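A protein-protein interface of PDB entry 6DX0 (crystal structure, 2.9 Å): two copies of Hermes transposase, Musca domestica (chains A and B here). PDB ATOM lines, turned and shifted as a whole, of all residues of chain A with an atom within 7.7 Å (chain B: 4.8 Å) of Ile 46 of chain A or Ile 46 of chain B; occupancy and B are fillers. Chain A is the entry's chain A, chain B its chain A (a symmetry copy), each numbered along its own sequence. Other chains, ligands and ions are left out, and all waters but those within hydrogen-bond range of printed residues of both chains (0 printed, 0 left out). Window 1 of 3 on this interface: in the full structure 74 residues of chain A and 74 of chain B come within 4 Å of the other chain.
Ile 46 of chain A touches just these residues of chain B: Ile 46 (3.7 Å) and Phe 49 (3.3 Å).
Of the printed residues of chain B, Lys 47 of chain A touches Val 62.
Of the printed residues of chain B, Phe 49 of chain A touches Ile 46 (3.3 Å), Phe 49 (3.3 Å) and Ile 50 (3.1 Å).
Lys 51 of chain A touches none of the printed residues of chain B.
Of the printed residues of chain B, Val 62 of chain A touches Lys 47.
Leu 65 of chain A touches none of the printed residues of chain B.
Printed residues of chain A within 4 Å of Ile 43 of chain B: Leu 66.
Printed residues of chain A within 4 Å of Met 45 of chain B: Lys 22 (3.6 Å), Cys 23 (3.97 Å), Trp 26 (3.96 Å) and Phe 42 (3.97 Å).
Of chain A, only Ile 46 (3.7 Å) and Phe 49 (3.3 Å) come within 4 Å of Ile 46 of chain B.
The nearest residue of chain A that does not touch Ile 46 of chain B is Val 62 of chain A (4.3 Å).
CD of Lys 22 of chain A touches O of Asp 44 of chain B, 3.7 Å away.
Cys 23 of chain A touches Met 45 of chain B.
CZ of Phe 42 of chain A touches SD of Met 45 of chain B, at 3.97 Å.
Ile 46 of chain A touches Ile 46 of chain B (CD1 to CD1, 3.7 Å).
CD2 of Phe 49 of chain B touches CD1 of Ile 46 of chain A (3.3 Å).
Lys 47 of chain A touches Val 62 of chain B (CE to CG2, 3.5 Å).
Phe 49 of chain A touches Ile 46 of chain B.
Phe 49 of chain A touches Ile 50 of chain B (O to CG2, 3.1 Å).
Val 62 of chain A touches Lys 47 of chain B (CG2 to CE, 3.5 Å).
Ile 43 of chain B touches Leu 66 of chain A.
Of the 10 printed residues of chain B, 10 touch a printed residue of chain A.
Hydrophobic or aromatic side chains of chain B that line the printed part of chain A: Phe 42, Ile 43, Met 45, Ile 46, Phe 48, Phe 49, Ile 50 and Val 62.
Of the 20 printed residues of chain A, 12 touch a printed residue of chain B.
Printed residues of chain A that touch a printed residue of chain B: Lys 22, Cys 23, Trp 26, Phe 42, Met 45, Ile 46, Lys 47, Phe 49, Ile 50, Gly 53, Val 62 and Leu 66.
Hydrophobic or aromatic side chains of chain A that line the printed part of chain B: Trp 26, Phe 42, Met 45, Ile 46, Phe 49, Ile 50, Val 62 and Leu 66.
Among the printed residues, 18 pairs touch across the chains.
O of Phe 49 of chain B sits close to O of Phe 49 of chain A (3.3 Å).
Phe 42 of chain A touches Met 45 of chain B, and with the chains exchanged Met 45 of chain A touches Phe 42 of chain B.
Ile 46 of chain A touches Phe 49 of chain B, and with the chains exchanged Phe 49 of chain A touches Ile 46 of chain B.
Lys 47 of chain A touches Val 62 of chain B, and with the chains exchanged Val 62 of chain A touches Lys 47 of chain B.
Phe 49 of chain A touches Ile 50 of chain B, and with the chains exchanged Ile 50 of chain A touches Phe 49 of chain B.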
ATOM      1  N   LYS A  22     -10.819  -8.272  23.674  1.00  0.00           N
ATOM      2  CA  LYS A  22      -9.597  -7.499  23.490  1.00  0.00           C
ATOM      3  C   LYS A  22      -9.299  -6.591  24.675  1.00  0.00           C
ATOM      4  O   LYS A  22      -8.136  -6.223  24.892  1.00  0.00           O
ATOM      5  CB  LYS A  22      -9.684  -6.657  22.204  1.00  0.00           C
ATOM      6  CG  LYS A  22      -9.750  -7.475  20.909  1.00  0.00           C
ATOM      7  CD  LYS A  22      -8.403  -7.584  20.192  1.00  0.00           C
ATOM      8  CE  LYS A  22      -7.957  -9.036  20.037  1.00  0.00           C
ATOM      9  NZ  LYS A  22      -9.061  -9.939  19.618  1.00  0.00           N
ATOM     10  N   CYS A  23     -10.320  -6.225  25.445  1.00  0.00           N
ATOM     11  CA  CYS A  23     -10.092  -5.437  26.646  1.00  0.00           C
ATOM     12  C   CYS A  23      -9.505  -6.292  27.766  1.00  0.00           C
ATOM     13  O   CYS A  23      -8.542  -5.890  28.433  1.00  0.00           O
ATOM     14  CB  CYS A  23     -11.400  -4.788  27.075  1.00  0.00           C
ATOM     15  SG  CYS A  23     -11.798  -3.405  26.044  1.00  0.00           S
ATOM     16  N   TRP A  26      -5.892  -6.489  27.245  1.00  0.00           N
ATOM     17  CA  TRP A  26      -5.161  -5.303  27.654  1.00  0.00           C
ATOM     18  C   TRP A  26      -4.785  -5.381  29.120  1.00  0.00           C
ATOM     19  O   TRP A  26      -3.665  -5.035  29.515  1.00  0.00           O
ATOM     20  CB  TRP A  26      -6.037  -4.094  27.418  1.00  0.00           C
ATOM     21  CG  TRP A  26      -5.475  -2.835  27.868  1.00  0.00           C
ATOM     22  CD1 TRP A  26      -4.189  -2.416  27.741  1.00  0.00           C
ATOM     23  CD2 TRP A  26      -6.188  -1.783  28.504  1.00  0.00           C
ATOM     24  NE1 TRP A  26      -4.054  -1.155  28.266  1.00  0.00           N
ATOM     25  CE2 TRP A  26      -5.275  -0.746  28.739  1.00  0.00           C
ATOM     26  CE3 TRP A  26      -7.514  -1.616  28.895  1.00  0.00           C
ATOM     27  CZ2 TRP A  26      -5.644   0.444  29.346  1.00  0.00           C
ATOM     28  CZ3 TRP A  26      -7.877  -0.443  29.507  1.00  0.00           C
ATOM     29  CH2 TRP A  26      -6.950   0.576  29.721  1.00  0.00           C
ATOM     30  N   VAL A  37     -11.182   0.668  31.840  1.00  0.00           N
ATOM     31  CA  VAL A  37     -12.209   0.667  30.809  1.00  0.00           C
ATOM     32  C   VAL A  37     -13.320   1.672  31.080  1.00  0.00           C
ATOM     33  O   VAL A  37     -14.034   2.074  30.153  1.00  0.00           O
ATOM     34  CB  VAL A  37     -12.788  -0.756  30.690  1.00  0.00           C
ATOM     35  CG1 VAL A  37     -13.498  -1.120  31.973  1.00  0.00           C
ATOM     36  CG2 VAL A  37     -13.726  -0.870  29.482  1.00  0.00           C
ATOM     37  N   GLY A  41     -11.486   9.645  30.685  1.00  0.00           N
ATOM     38  CA  GLY A  41     -10.480   9.942  29.681  1.00  0.00           C
ATOM     39  C   GLY A  41     -10.229   8.793  28.733  1.00  0.00           C
ATOM     40  O   GLY A  41      -9.856   9.008  27.577  1.00  0.00           O
ATOM     41  N   PHE A  42     -10.415   7.564  29.201  1.00  0.00           N
ATOM     42  CA  PHE A  42     -10.175   6.418  28.338  1.00  0.00           C
ATOM     43  C   PHE A  42     -11.195   6.338  27.216  1.00  0.00           C
ATOM     44  O   PHE A  42     -10.875   5.874  26.114  1.00  0.00           O
ATOM     45  CB  PHE A  42     -10.217   5.143  29.151  1.00  0.00           C
ATOM     46  CG  PHE A  42     -10.095   3.897  28.328  1.00  0.00           C
ATOM     47  CD1 PHE A  42      -8.878   3.532  27.782  1.00  0.00           C
ATOM     48  CD2 PHE A  42     -11.190   3.074  28.125  1.00  0.00           C
ATOM     49  CE1 PHE A  42      -8.751   2.371  27.041  1.00  0.00           C
ATOM     50  CE2 PHE A  42     -11.075   1.907  27.385  1.00  0.00           C
ATOM     51  CZ  PHE A  42      -9.852   1.556  26.839  1.00  0.00           C
ATOM     52  N   ILE A  43     -12.427   6.776  27.476  1.00  0.00           N
ATOM     53  CA  ILE A  43     -13.476   6.643  26.471  1.00  0.00           C
ATOM     54  C   ILE A  43     -13.251   7.634  25.335  1.00  0.00           C
ATOM     55  O   ILE A  43     -13.242   7.255  24.158  1.00  0.00           O
ATOM     56  CB  ILE A  43     -14.863   6.813  27.114  1.00  0.00           C
ATOM     57  CG1 ILE A  43     -15.103   5.717  28.157  1.00  0.00           C
ATOM     58  CG2 ILE A  43     -15.942   6.780  26.046  1.00  0.00           C
ATOM     59  CD1 ILE A  43     -16.518   5.683  28.695  1.00  0.00           C
ATOM     60  N   ASP A  44     -13.042   8.914  25.673  1.00  0.00           N
ATOM     61  CA  ASP A  44     -12.769   9.926  24.656  1.00  0.00           C
ATOM     62  C   ASP A  44     -11.583   9.544  23.784  1.00  0.00           C
ATOM     63  O   ASP A  44     -11.503   9.963  22.622  1.00  0.00           O
ATOM     64  CB  ASP A  44     -12.514  11.284  25.311  1.00  0.00           C
ATOM     65  CG  ASP A  44     -13.608  11.676  26.283  1.00  0.00           C
ATOM     66  OD1 ASP A  44     -14.501  10.839  26.543  1.00  0.00           O
ATOM     67  OD2 ASP A  44     -13.564  12.815  26.802  1.00  0.00           O
ATOM     68  N   MET A  45     -10.658   8.755  24.321  1.00  0.00           N
ATOM     69  CA  MET A  45      -9.521   8.279  23.549  1.00  0.00           C
ATOM     70  C   MET A  45      -9.873   7.076  22.683  1.00  0.00           C
ATOM     71  O   MET A  45      -9.097   6.723  21.789  1.00  0.00           O
ATOM     72  CB  MET A  45      -8.362   7.940  24.493  1.00  0.00           C
ATOM     73  CG  MET A  45      -7.023   7.802  23.797  1.00  0.00           C
ATOM     74  SD  MET A  45      -6.017   6.472  24.472  1.00  0.00           S
ATOM     75  CE  MET A  45      -7.272   5.257  24.892  1.00  0.00           C
ATOM     76  N   ILE A  46     -11.015   6.440  22.921  1.00  0.00           N
ATOM     77  CA  ILE A  46     -11.487   5.405  22.006  1.00  0.00           C
ATOM     78  C   ILE A  46     -12.405   5.997  20.936  1.00  0.00           C
ATOM     79  O   ILE A  46     -12.411   5.529  19.793  1.00  0.00           O
ATOM     80  CB  ILE A  46     -12.174   4.276  22.796  1.00  0.00           C
ATOM     81  CG1 ILE A  46     -11.138   3.529  23.635  1.00  0.00           C
ATOM     82  CG2 ILE A  46     -12.899   3.325  21.870  1.00  0.00           C
ATOM     83  CD1 ILE A  46      -9.814   3.339  22.928  1.00  0.00           C
ATOM     84  N   LYS A  47     -13.166   7.034  21.298  1.00  0.00           N
ATOM     85  CA  LYS A  47     -13.875   7.857  20.326  1.00  0.00           C
ATOM     86  C   LYS A  47     -12.950   8.276  19.198  1.00  0.00           C
ATOM     87  O   LYS A  47     -13.317   8.216  18.014  1.00  0.00           O
ATOM     88  CB  LYS A  47     -14.453   9.091  21.013  1.00  0.00           C
ATOM     89  CG  LYS A  47     -15.538   8.778  22.012  1.00  0.00           C
ATOM     90  CD  LYS A  47     -16.202  10.046  22.494  1.00  0.00           C
ATOM     91  CE  LYS A  47     -17.352   9.721  23.432  1.00  0.00           C
ATOM     92  NZ  LYS A  47     -18.422  10.756  23.412  1.00  0.00           N
ATOM     93  N   PHE A  48     -11.735   8.696  19.552  1.00  0.00           N
ATOM     94  CA  PHE A  48     -10.803   9.155  18.538  1.00  0.00           C
ATOM     95  C   PHE A  48     -10.309   8.017  17.657  1.00  0.00           C
ATOM     96  O   PHE A  48     -10.032   8.231  16.475  1.00  0.00           O
ATOM     97  CB  PHE A  48      -9.630   9.853  19.198  1.00  0.00           C
ATOM     98  CG  PHE A  48      -8.554  10.228  18.240  1.00  0.00           C
ATOM     99  CD1 PHE A  48      -8.664  11.369  17.472  1.00  0.00           C
ATOM    100  CD2 PHE A  48      -7.431   9.435  18.099  1.00  0.00           C
ATOM    101  CE1 PHE A  48      -7.677  11.712  16.588  1.00  0.00           C
ATOM    102  CE2 PHE A  48      -6.440   9.773  17.213  1.00  0.00           C
ATOM    103  CZ  PHE A  48      -6.563  10.913  16.458  1.00  0.00           C
ATOM    104  N   PHE A  49     -10.189   6.806  18.202  1.00  0.00           N
ATOM    105  CA  PHE A  49      -9.613   5.710  17.432  1.00  0.00           C
ATOM    106  C   PHE A  49     -10.630   4.979  16.574  1.00  0.00           C
ATOM    107  O   PHE A  49     -10.243   4.323  15.605  1.00  0.00           O
ATOM    108  CB  PHE A  49      -8.921   4.716  18.362  1.00  0.00           C
ATOM    109  CG  PHE A  49      -7.584   5.189  18.846  1.00  0.00           C
ATOM    110  CD1 PHE A  49      -6.894   6.172  18.156  1.00  0.00           C
ATOM    111  CD2 PHE A  49      -7.018   4.662  19.989  1.00  0.00           C
ATOM    112  CE1 PHE A  49      -5.663   6.614  18.595  1.00  0.00           C
ATOM    113  CE2 PHE A  49      -5.791   5.091  20.426  1.00  0.00           C
ATOM    114  CZ  PHE A  49      -5.112   6.076  19.733  1.00  0.00           C
ATOM    115  N   ILE A  50     -11.914   5.043  16.914  1.00  0.00           N
ATOM    116  CA  ILE A  50     -12.914   4.530  15.990  1.00  0.00           C
ATOM    117  C   ILE A  50     -13.104   5.509  14.839  1.00  0.00           C
ATOM    118  O   ILE A  50     -13.213   5.108  13.675  1.00  0.00           O
ATOM    119  CB  ILE A  50     -14.232   4.234  16.731  1.00  0.00           C
ATOM    120  CG1 ILE A  50     -14.693   5.456  17.535  1.00  0.00           C
ATOM    121  CG2 ILE A  50     -14.059   3.036  17.665  1.00  0.00           C
ATOM    122  CD1 ILE A  50     -15.747   6.314  16.850  1.00  0.00           C
ATOM    123  N   LYS A  51     -13.109   6.811  15.145  1.00  0.00           N
ATOM    124  CA  LYS A  51     -13.211   7.833  14.108  1.00  0.00           C
ATOM    125  C   LYS A  51     -12.106   7.671  13.078  1.00  0.00           C
ATOM    126  O   LYS A  51     -12.365   7.619  11.873  1.00  0.00           O
ATOM    127  CB  LYS A  51     -13.151   9.228  14.735  1.00  0.00           C
ATOM    128  CG  LYS A  51     -12.484  10.280  13.854  1.00  0.00           C
ATOM    129  CD  LYS A  51     -12.544  11.659  14.488  1.00  0.00           C
ATOM    130  CE  LYS A  51     -11.980  12.741  13.566  1.00  0.00           C
ATOM    131  NZ  LYS A  51     -10.552  12.535  13.190  1.00  0.00           N
ATOM    132  N   VAL A  52     -10.863   7.582  13.543  1.00  0.00           N
ATOM    133  CA  VAL A  52      -9.734   7.418  12.638  1.00  0.00           C
ATOM    134  C   VAL A  52      -9.849   6.104  11.874  1.00  0.00           C
ATOM    135  O   VAL A  52      -9.546   6.037  10.676  1.00  0.00           O
ATOM    136  CB  VAL A  52      -8.418   7.531  13.431  1.00  0.00           C
ATOM    137  CG1 VAL A  52      -7.291   6.747  12.775  1.00  0.00           C
ATOM    138  CG2 VAL A  52      -8.046   8.992  13.597  1.00  0.00           C
ATOM    139  N   GLY A  53     -10.315   5.047  12.538  1.00  0.00           N
ATOM    140  CA  GLY A  53     -10.556   3.804  11.822  1.00  0.00           C
ATOM    141  C   GLY A  53     -11.551   3.980  10.689  1.00  0.00           C
ATOM    142  O   GLY A  53     -11.318   3.535   9.560  1.00  0.00           O
ATOM    143  N   VAL A  62      -0.504   1.244  13.350  1.00  0.00           N
ATOM    144  CA  VAL A  62      -0.752   1.534  14.763  1.00  0.00           C
ATOM    145  C   VAL A  62       0.525   2.019  15.444  1.00  0.00           C
ATOM    146  O   VAL A  62       0.548   3.096  16.052  1.00  0.00           O
ATOM    147  CB  VAL A  62      -1.341   0.298  15.468  1.00  0.00           C
ATOM    148  CG1 VAL A  62      -2.863   0.395  15.539  1.00  0.00           C
ATOM    149  CG2 VAL A  62      -0.925  -0.975  14.743  1.00  0.00           C
ATOM    150  N   LEU A  65       1.609   5.563  14.278  1.00  0.00           N
ATOM    151  CA  LEU A  65       0.630   6.565  14.679  1.00  0.00           C
ATOM    152  C   LEU A  65       0.540   6.709  16.199  1.00  0.00           C
ATOM    153  O   LEU A  65       0.312   7.821  16.694  1.00  0.00           O
ATOM    154  CB  LEU A  65      -0.721   6.207  14.055  1.00  0.00           C
ATOM    155  CG  LEU A  65      -2.110   6.161  14.707  1.00  0.00           C
ATOM    156  CD1 LEU A  65      -2.230   5.043  15.766  1.00  0.00           C
ATOM    157  CD2 LEU A  65      -2.555   7.534  15.233  1.00  0.00           C
ATOM    158  N   LEU A  66       0.721   5.610  16.948  1.00  0.00           N
ATOM    159  CA  LEU A  66       0.672   5.674  18.410  1.00  0.00           C
ATOM    160  C   LEU A  66       1.852   6.479  18.933  1.00  0.00           C
ATOM    161  O   LEU A  66       2.993   6.240  18.517  1.00  0.00           O
ATOM    162  CB  LEU A  66       0.685   4.280  19.039  1.00  0.00           C
ATOM    163  CG  LEU A  66      -0.701   3.698  19.350  1.00  0.00           C
ATOM    164  CD1 LEU A  66      -0.611   2.304  19.963  1.00  0.00           C
ATOM    165  CD2 LEU A  66      -1.527   4.659  20.222  1.00  0.00           C
ATOM    166  N   PHE B  42      -1.976  -3.022  24.914  1.00  0.00           N
ATOM    167  CA  PHE B  42      -2.721  -1.809  24.617  1.00  0.00           C
ATOM    168  C   PHE B  42      -2.839  -1.576  23.121  1.00  0.00           C
ATOM    169  O   PHE B  42      -3.842  -1.021  22.654  1.00  0.00           O
ATOM    170  CB  PHE B  42      -2.045  -0.619  25.261  1.00  0.00           C
ATOM    171  CG  PHE B  42      -2.675   0.696  24.915  1.00  0.00           C
ATOM    172  CD1 PHE B  42      -3.889   1.061  25.469  1.00  0.00           C
ATOM    173  CD2 PHE B  42      -2.041   1.581  24.060  1.00  0.00           C
ATOM    174  CE1 PHE B  42      -4.467   2.282  25.173  1.00  0.00           C
ATOM    175  CE2 PHE B  42      -2.610   2.808  23.756  1.00  0.00           C
ATOM    176  CZ  PHE B  42      -3.828   3.159  24.313  1.00  0.00           C
ATOM    177  N   ILE B  43      -1.827  -1.984  22.356  1.00  0.00           N
ATOM    178  CA  ILE B  43      -1.838  -1.710  20.923  1.00  0.00           C
ATOM    179  C   ILE B  43      -2.862  -2.594  20.222  1.00  0.00           C
ATOM    180  O   ILE B  43      -3.711  -2.103  19.468  1.00  0.00           O
ATOM    181  CB  ILE B  43      -0.429  -1.882  20.331  1.00  0.00           C
ATOM    182  CG1 ILE B  43       0.542  -0.885  20.969  1.00  0.00           C
ATOM    183  CG2 ILE B  43      -0.469  -1.700  18.824  1.00  0.00           C
ATOM    184  CD1 ILE B  43       1.903  -0.843  20.305  1.00  0.00           C
ATOM    185  N   ASP B  44      -2.813  -3.908  20.478  1.00  0.00           N
ATOM    186  CA  ASP B  44      -3.784  -4.827  19.890  1.00  0.00           C
ATOM    187  C   ASP B  44      -5.213  -4.412  20.201  1.00  0.00           C
ATOM    188  O   ASP B  44      -6.134  -4.718  19.432  1.00  0.00           O
ATOM    189  CB  ASP B  44      -3.538  -6.251  20.387  1.00  0.00           C
ATOM    190  CG  ASP B  44      -2.099  -6.690  20.208  1.00  0.00           C
ATOM    191  OD1 ASP B  44      -1.264  -5.845  19.815  1.00  0.00           O
ATOM    192  OD2 ASP B  44      -1.799  -7.875  20.480  1.00  0.00           O
ATOM    193  N   MET B  45      -5.420  -3.719  21.317  1.00  0.00           N
ATOM    194  CA  MET B  45      -6.739  -3.219  21.669  1.00  0.00           C
ATOM    195  C   MET B  45      -7.080  -1.923  20.944  1.00  0.00           C
ATOM    196  O   MET B  45      -8.246  -1.518  20.939  1.00  0.00           O
ATOM    197  CB  MET B  45      -6.828  -3.023  23.187  1.00  0.00           C
ATOM    198  CG  MET B  45      -8.243  -2.875  23.706  1.00  0.00           C
ATOM    199  SD  MET B  45      -8.382  -1.661  25.027  1.00  0.00           S
ATOM    200  CE  MET B  45      -7.167  -0.441  24.515  1.00  0.00           C
ATOM    201  N   ILE B  46      -6.099  -1.266  20.334  1.00  0.00           N
ATOM    202  CA  ILE B  46      -6.400  -0.127  19.472  1.00  0.00           C
ATOM    203  C   ILE B  46      -6.579  -0.573  18.020  1.00  0.00           C
ATOM    204  O   ILE B  46      -7.388   0.005  17.288  1.00  0.00           O
ATOM    205  CB  ILE B  46      -5.306   0.947  19.616  1.00  0.00           C
ATOM    206  CG1 ILE B  46      -5.371   1.565  21.012  1.00  0.00           C
ATOM    207  CG2 ILE B  46      -5.446   2.014  18.553  1.00  0.00           C
ATOM    208  CD1 ILE B  46      -6.782   1.766  21.518  1.00  0.00           C
ATOM    209  N   LYS B  47      -5.839  -1.606  17.609  1.00  0.00           N
ATOM    210  CA  LYS B  47      -6.099  -2.300  16.353  1.00  0.00           C
ATOM    211  C   LYS B  47      -7.571  -2.645  16.223  1.00  0.00           C
ATOM    212  O   LYS B  47      -8.182  -2.455  15.159  1.00  0.00           O
ATOM    213  CB  LYS B  47      -5.256  -3.569  16.276  1.00  0.00           C
ATOM    214  CG  LYS B  47      -3.773  -3.309  16.192  1.00  0.00           C
ATOM    215  CD  LYS B  47      -3.022  -4.589  15.911  1.00  0.00           C
ATOM    216  CE  LYS B  47      -1.539  -4.309  15.738  1.00  0.00           C
ATOM    217  NZ  LYS B  47      -0.866  -5.290  14.843  1.00  0.00           N
ATOM    218  N   PHE B  48      -8.161  -3.149  17.308  1.00  0.00           N
ATOM    219  CA  PHE B  48      -9.556  -3.546  17.256  1.00  0.00           C
ATOM    220  C   PHE B  48     -10.487  -2.349  17.131  1.00  0.00           C
ATOM    221  O   PHE B  48     -11.548  -2.458  16.511  1.00  0.00           O
ATOM    222  CB  PHE B  48      -9.905  -4.355  18.490  1.00  0.00           C
ATOM    223  CG  PHE B  48     -11.354  -4.679  18.590  1.00  0.00           C
ATOM    224  CD1 PHE B  48     -11.887  -5.734  17.878  1.00  0.00           C
ATOM    225  CD2 PHE B  48     -12.190  -3.925  19.390  1.00  0.00           C
ATOM    226  CE1 PHE B  48     -13.221  -6.031  17.966  1.00  0.00           C
ATOM    227  CE2 PHE B  48     -13.527  -4.216  19.481  1.00  0.00           C
ATOM    228  CZ  PHE B  48     -14.043  -5.271  18.768  1.00  0.00           C
ATOM    229  N   PHE B  49     -10.121  -1.204  17.705  1.00  0.00           N
ATOM    230  CA  PHE B  49     -11.028  -0.063  17.711  1.00  0.00           C
ATOM    231  C   PHE B  49     -10.929   0.791  16.460  1.00  0.00           C
ATOM    232  O   PHE B  49     -11.873   1.522  16.150  1.00  0.00           O
ATOM    233  CB  PHE B  49     -10.781   0.805  18.943  1.00  0.00           C
ATOM    234  CG  PHE B  49     -11.361   0.230  20.200  1.00  0.00           C
ATOM    235  CD1 PHE B  49     -12.377  -0.709  20.139  1.00  0.00           C
ATOM    236  CD2 PHE B  49     -10.891   0.618  21.438  1.00  0.00           C
ATOM    237  CE1 PHE B  49     -12.916  -1.243  21.292  1.00  0.00           C
ATOM    238  CE2 PHE B  49     -11.429   0.097  22.587  1.00  0.00           C
ATOM    239  CZ  PHE B  49     -12.440  -0.843  22.517  1.00  0.00           C
ATOM    240  N   ILE B  50      -9.807   0.748  15.748  1.00  0.00           N
ATOM    241  CA  ILE B  50      -9.776   1.391  14.442  1.00  0.00           C
ATOM    242  C   ILE B  50     -10.527   0.538  13.429  1.00  0.00           C
ATOM    243  O   ILE B  50     -11.285   1.055  12.601  1.00  0.00           O
ATOM    244  CB  ILE B  50      -8.323   1.669  14.013  1.00  0.00           C
ATOM    245  CG1 ILE B  50      -7.474   0.395  14.101  1.00  0.00           C
ATOM    246  CG2 ILE B  50      -7.709   2.762  14.887  1.00  0.00           C
ATOM    247  CD1 ILE B  50      -7.291  -0.347  12.785  1.00  0.00           C
ATOM    248  N   VAL B  62     -20.036   4.389  22.027  1.00  0.00           N
ATOM    249  CA  VAL B  62     -18.849   3.974  22.774  1.00  0.00           C
ATOM    250  C   VAL B  62     -19.244   3.371  24.120  1.00  0.00           C
ATOM    251  O   VAL B  62     -18.862   2.240  24.443  1.00  0.00           O
ATOM    252  CB  VAL B  62     -17.880   5.159  22.943  1.00  0.00           C
ATOM    253  CG1 VAL B  62     -16.793   5.120  21.872  1.00  0.00           C
ATOM    254  CG2 VAL B  62     -18.639   6.478  22.880  1.00  0.00           C
